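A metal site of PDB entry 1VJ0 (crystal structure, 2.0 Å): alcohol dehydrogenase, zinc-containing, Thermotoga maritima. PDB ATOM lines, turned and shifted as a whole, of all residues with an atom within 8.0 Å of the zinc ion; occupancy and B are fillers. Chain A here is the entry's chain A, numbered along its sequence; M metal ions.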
ATOM      1  N   ILE A 110      -7.983 -10.357  14.937  1.00  0.00           N
ATOM      2  CA  ILE A 110      -9.159 -10.162  15.788  1.00  0.00           C
ATOM      3  C   ILE A 110      -8.858 -10.930  17.065  1.00  0.00           C
ATOM      4  O   ILE A 110      -8.378 -12.053  17.022  1.00  0.00           O
ATOM      5  CB  ILE A 110     -10.402 -10.758  15.131  1.00  0.00           C
ATOM      6  CG1 ILE A 110     -10.797  -9.954  13.862  1.00  0.00           C
ATOM      7  CG2 ILE A 110     -11.581 -10.841  16.148  1.00  0.00           C
ATOM      8  CD1 ILE A 110     -12.008 -10.551  13.178  1.00  0.00           C
ATOM      9  N   THR A 111      -9.045 -10.253  18.180  1.00  0.00           N
ATOM     10  CA  THR A 111      -8.786 -10.837  19.499  1.00  0.00           C
ATOM     11  C   THR A 111     -10.134 -11.102  20.148  1.00  0.00           C
ATOM     12  O   THR A 111     -11.143 -10.623  19.677  1.00  0.00           O
ATOM     13  CB  THR A 111      -7.880  -9.878  20.355  1.00  0.00           C
ATOM     14  OG1 THR A 111      -8.517  -8.614  20.605  1.00  0.00           O
ATOM     15  CG2 THR A 111      -6.607  -9.532  19.581  1.00  0.00           C
ATOM     16  N   CYS A 112     -10.133 -11.853  21.223  1.00  0.00           N
ATOM     17  CA  CYS A 112     -11.362 -12.331  21.844  1.00  0.00           C
ATOM     18  C   CYS A 112     -12.130 -11.271  22.620  1.00  0.00           C
ATOM     19  O   CYS A 112     -13.357 -11.346  22.689  1.00  0.00           O
ATOM     20  CB  CYS A 112     -11.109 -13.569  22.678  1.00  0.00           C
ATOM     21  SG  CYS A 112     -10.300 -13.351  24.298  1.00  0.00           S
ATOM     22  N   GLY A 113     -11.434 -10.275  23.164  1.00  0.00           N
ATOM     23  CA  GLY A 113     -12.085  -9.285  23.973  1.00  0.00           C
ATOM     24  C   GLY A 113     -12.602  -9.766  25.317  1.00  0.00           C
ATOM     25  O   GLY A 113     -13.374  -9.030  25.938  1.00  0.00           O
ATOM     26  N   GLU A 114     -12.113 -10.914  25.798  1.00  0.00           N
ATOM     27  CA  GLU A 114     -12.607 -11.581  27.008  1.00  0.00           C
ATOM     28  C   GLU A 114     -11.499 -12.103  27.945  1.00  0.00           C
ATOM     29  O   GLU A 114     -11.760 -12.387  29.106  1.00  0.00           O
ATOM     30  CB  GLU A 114     -13.545 -12.719  26.624  1.00  0.00           C
ATOM     31  CG  GLU A 114     -14.740 -12.186  25.840  1.00  0.00           C
ATOM     32  CD  GLU A 114     -15.829 -13.198  25.726  1.00  0.00           C
ATOM     33  OE1 GLU A 114     -15.500 -14.356  25.364  1.00  0.00           O
ATOM     34  OE2 GLU A 114     -17.009 -12.826  26.000  1.00  0.00           O
ATOM     35  N   CYS A 115     -10.265 -12.213  27.470  1.00  0.00           N
ATOM     36  CA  CYS A 115      -9.250 -12.868  28.258  1.00  0.00           C
ATOM     37  C   CYS A 115      -8.467 -11.863  29.109  1.00  0.00           C
ATOM     38  O   CYS A 115      -8.671 -10.642  29.033  1.00  0.00           O
ATOM     39  CB  CYS A 115      -8.314 -13.650  27.360  1.00  0.00           C
ATOM     40  SG  CYS A 115      -7.271 -12.596  26.384  1.00  0.00           S
ATOM     41  N   TYR A 116      -7.563 -12.406  29.904  1.00  0.00           N
ATOM     42  CA  TYR A 116      -6.668 -11.620  30.738  1.00  0.00           C
ATOM     43  C   TYR A 116      -5.947 -10.548  29.933  1.00  0.00           C
ATOM     44  O   TYR A 116      -5.821  -9.411  30.367  1.00  0.00           O
ATOM     45  CB  TYR A 116      -5.625 -12.511  31.402  1.00  0.00           C
ATOM     46  CG  TYR A 116      -4.581 -11.786  32.239  1.00  0.00           C
ATOM     47  CD1 TYR A 116      -4.823 -11.437  33.579  1.00  0.00           C
ATOM     48  CD2 TYR A 116      -3.381 -11.401  31.683  1.00  0.00           C
ATOM     49  CE1 TYR A 116      -3.883 -10.775  34.325  1.00  0.00           C
ATOM     50  CE2 TYR A 116      -2.447 -10.730  32.421  1.00  0.00           C
ATOM     51  CZ  TYR A 116      -2.678 -10.423  33.732  1.00  0.00           C
ATOM     52  OH  TYR A 116      -1.672  -9.786  34.458  1.00  0.00           O
ATOM     53  N   TRP A 117      -5.441 -10.928  28.761  1.00  0.00           N
ATOM     54  CA  TRP A 117      -4.651  -9.991  27.993  1.00  0.00           C
ATOM     55  C   TRP A 117      -5.500  -8.912  27.351  1.00  0.00           C
ATOM     56  O   TRP A 117      -5.079  -7.729  27.335  1.00  0.00           O
ATOM     57  CB  TRP A 117      -3.767 -10.685  26.972  1.00  0.00           C
ATOM     58  CG  TRP A 117      -2.646 -11.464  27.587  1.00  0.00           C
ATOM     59  CD1 TRP A 117      -1.413 -10.997  27.959  1.00  0.00           C
ATOM     60  CD2 TRP A 117      -2.651 -12.853  27.935  1.00  0.00           C
ATOM     61  NE1 TRP A 117      -0.658 -12.022  28.487  1.00  0.00           N
ATOM     62  CE2 TRP A 117      -1.382 -13.165  28.458  1.00  0.00           C
ATOM     63  CE3 TRP A 117      -3.608 -13.886  27.810  1.00  0.00           C
ATOM     64  CZ2 TRP A 117      -1.042 -14.446  28.917  1.00  0.00           C
ATOM     65  CZ3 TRP A 117      -3.261 -15.166  28.275  1.00  0.00           C
ATOM     66  CH2 TRP A 117      -1.993 -15.431  28.779  1.00  0.00           C
ATOM     67  N   CYS A 118      -6.649  -9.287  26.785  1.00  0.00           N
ATOM     68  CA  CYS A 118      -7.549  -8.333  26.191  1.00  0.00           C
ATOM     69  C   CYS A 118      -8.176  -7.409  27.264  1.00  0.00           C
ATOM     70  O   CYS A 118      -8.371  -6.250  27.009  1.00  0.00           O
ATOM     71  CB  CYS A 118      -8.660  -9.030  25.462  1.00  0.00           C
ATOM     72  SG  CYS A 118      -8.156  -9.944  23.943  1.00  0.00           S
ATOM     73  N   LYS A 119      -8.480  -7.920  28.452  1.00  0.00           N
ATOM     74  CA  LYS A 119      -9.301  -7.147  29.412  1.00  0.00           C
ATOM     75  C   LYS A 119      -8.595  -6.658  30.672  1.00  0.00           C
ATOM     76  O   LYS A 119      -9.065  -5.715  31.283  1.00  0.00           O
ATOM     77  CB  LYS A 119     -10.562  -7.923  29.810  1.00  0.00           C
ATOM     78  CG  LYS A 119     -11.661  -7.902  28.730  1.00  0.00           C
ATOM     79  CD  LYS A 119     -12.375  -6.513  28.785  1.00  0.00           C
ATOM     80  CE  LYS A 119     -13.547  -6.384  27.831  1.00  0.00           C
ATOM     81  NZ  LYS A 119     -14.565  -7.474  27.968  1.00  0.00           N
ATOM     82  N   GLU A 123      -3.131  -5.849  26.693  1.00  0.00           N
ATOM     83  CA  GLU A 123      -2.157  -6.256  25.695  1.00  0.00           C
ATOM     84  C   GLU A 123      -2.801  -7.225  24.699  1.00  0.00           C
ATOM     85  O   GLU A 123      -2.440  -8.390  24.637  1.00  0.00           O
ATOM     86  CB  GLU A 123      -0.990  -6.965  26.395  1.00  0.00           C
ATOM     87  CG  GLU A 123      -0.233  -6.104  27.398  1.00  0.00           C
ATOM     88  CD  GLU A 123       0.576  -6.882  28.431  1.00  0.00           C
ATOM     89  OE1 GLU A 123       0.182  -7.976  28.901  1.00  0.00           O
ATOM     90  OE2 GLU A 123       1.619  -6.353  28.822  1.00  0.00           O
ATOM     91  N   PRO A 124      -3.739  -6.735  23.887  1.00  0.00           N
ATOM     92  CA  PRO A 124      -4.484  -7.611  22.989  1.00  0.00           C
ATOM     93  C   PRO A 124      -3.652  -8.337  21.941  1.00  0.00           C
ATOM     94  O   PRO A 124      -4.066  -9.407  21.491  1.00  0.00           O
ATOM     95  CB  PRO A 124      -5.485  -6.661  22.295  1.00  0.00           C
ATOM     96  CG  PRO A 124      -5.211  -5.306  22.795  1.00  0.00           C
ATOM     97  CD  PRO A 124      -4.142  -5.333  23.764  1.00  0.00           C
ATOM     98  N   TYR A 125      -2.490  -7.795  21.597  1.00  0.00           N
ATOM     99  CA  TYR A 125      -1.554  -8.479  20.675  1.00  0.00           C
ATOM    100  C   TYR A 125      -1.137  -9.811  21.288  1.00  0.00           C
ATOM    101  O   TYR A 125      -0.679 -10.739  20.572  1.00  0.00           O
ATOM    102  CB  TYR A 125      -0.334  -7.560  20.323  1.00  0.00           C
ATOM    103  CG  TYR A 125       0.200  -6.764  21.471  1.00  0.00           C
ATOM    104  CD1 TYR A 125      -0.332  -5.509  21.815  1.00  0.00           C
ATOM    105  CD2 TYR A 125       1.184  -7.280  22.288  1.00  0.00           C
ATOM    106  CE1 TYR A 125       0.119  -4.835  22.934  1.00  0.00           C
ATOM    107  CE2 TYR A 125       1.660  -6.614  23.391  1.00  0.00           C
ATOM    108  CZ  TYR A 125       1.097  -5.409  23.730  1.00  0.00           C
ATOM    109  OH  TYR A 125       1.608  -4.813  24.859  1.00  0.00           O
ATOM    110  N   LEU A 126      -1.256  -9.953  22.617  1.00  0.00           N
ATOM    111  CA  LEU A 126      -0.909 -11.228  23.288  1.00  0.00           C
ATOM    112  C   LEU A 126      -2.086 -12.228  23.520  1.00  0.00           C
ATOM    113  O   LEU A 126      -1.923 -13.273  24.136  1.00  0.00           O
ATOM    114  CB  LEU A 126      -0.179 -10.993  24.622  1.00  0.00           C
ATOM    115  CG  LEU A 126       1.053 -10.110  24.565  1.00  0.00           C
ATOM    116  CD1 LEU A 126       1.681  -9.846  25.918  1.00  0.00           C
ATOM    117  CD2 LEU A 126       2.032 -10.684  23.608  1.00  0.00           C
ATOM    118  N   CYS A 127      -3.243 -11.915  22.976  1.00  0.00           N
ATOM    119  CA  CYS A 127      -4.433 -12.738  23.159  1.00  0.00           C
ATOM    120  C   CYS A 127      -4.116 -14.139  22.593  1.00  0.00           C
ATOM    121  O   CYS A 127      -3.631 -14.270  21.481  1.00  0.00           O
ATOM    122  CB  CYS A 127      -5.570 -12.110  22.407  1.00  0.00           C
ATOM    123  SG  CYS A 127      -7.064 -13.141  22.326  1.00  0.00           S
ATOM    124  N   PRO A 128      -4.311 -15.198  23.366  1.00  0.00           N
ATOM    125  CA  PRO A 128      -4.056 -16.536  22.848  1.00  0.00           C
ATOM    126  C   PRO A 128      -5.092 -16.999  21.789  1.00  0.00           C
ATOM    127  O   PRO A 128      -4.920 -18.066  21.225  1.00  0.00           O
ATOM    128  CB  PRO A 128      -4.126 -17.416  24.102  1.00  0.00           C
ATOM    129  CG  PRO A 128      -5.023 -16.638  25.082  1.00  0.00           C
ATOM    130  CD  PRO A 128      -4.825 -15.191  24.737  1.00  0.00           C
ATOM    131  N   ASN A 129      -6.163 -16.243  21.570  1.00  0.00           N
ATOM    132  CA  ASN A 129      -7.256 -16.686  20.708  1.00  0.00           C
ATOM    133  C   ASN A 129      -7.277 -15.807  19.479  1.00  0.00           C
ATOM    134  O   ASN A 129      -8.307 -15.659  18.857  1.00  0.00           O
ATOM    135  CB  ASN A 129      -8.589 -16.529  21.456  1.00  0.00           C
ATOM    136  CG  ASN A 129      -8.653 -17.333  22.763  1.00  0.00           C
ATOM    137  OD1 ASN A 129      -8.466 -18.536  22.741  1.00  0.00           O
ATOM    138  ND2 ASN A 129      -8.962 -16.666  23.895  1.00  0.00           N
ATOM    139  N   ARG A 130      -6.151 -15.200  19.162  1.00  0.00           N
ATOM    140  CA  ARG A 130      -6.053 -14.197  18.065  1.00  0.00           C
ATOM    141  C   ARG A 130      -6.186 -14.874  16.675  1.00  0.00           C
ATOM    142  O   ARG A 130      -5.513 -15.861  16.387  1.00  0.00           O
ATOM    143  CB  ARG A 130      -4.700 -13.477  18.198  1.00  0.00           C
ATOM    144  CG  ARG A 130      -4.460 -12.293  17.333  1.00  0.00           C
ATOM    145  CD  ARG A 130      -3.191 -11.469  17.728  1.00  0.00           C
ATOM    146  NE  ARG A 130      -2.884 -10.596  16.641  1.00  0.00           N
ATOM    147  CZ  ARG A 130      -2.104 -10.916  15.597  1.00  0.00           C
ATOM    148  NH1 ARG A 130      -1.470 -12.097  15.534  1.00  0.00           N
ATOM    149  NH2 ARG A 130      -1.967 -10.039  14.629  1.00  0.00           N
HETATM  150 ZN    ZN M   1      -8.184 -12.253  24.243  1.00  0.00          ZN
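The side-chain sulfur (SG) of Cys 118 sits close to the backbone NH (N) of Gly 113, 3.4 Å away. SG of Cys 118 lies close to OG1 of Thr 111 (3.6 Å). The side-chain sulfur (SG) of Cys 115 lies close to the backbone NH (N) of Trp 117, at 3.4 Å. The backbone NH of Glu 114 lies close to the side-chain sulfur of Cys 112. The side-chain sulfur (SG) of Cys 112 sits close to the side-chain amide nitrogen (ND2) of Asn 129, 3.6 Å away. The side-chain sulfur (SG) of Cys 127 lies close to the backbone NH (N) of Asn 129 (3.3 Å). The side-chain amino group (NZ) of Lys 119 sits at hydrogen-bond distance from the backbone carbonyl oxygen (O) of Gly 113, at 2.8 Å.
Gly 113 touches the zinc ion. Five residues have an atom within 4 Å of the zinc ion: Cys 112, Gly 113, Cys 115, Cys 118 and Cys 127. Along chain A the residues within 4 Å of the zinc ion span positions 112 to 127. The nearest printed residue that does not touch the zinc ion is Glu 114 (4.4 Å).
The zinc ion is bound by the side-chain sulfur of Cys 118 (2.3 Å), the side-chain sulfur of Cys 115 (2.4 Å), the side-chain sulfur of Cys 112 (2.4 Å) and the side-chain sulfur of Cys 127 (2.4 Å).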
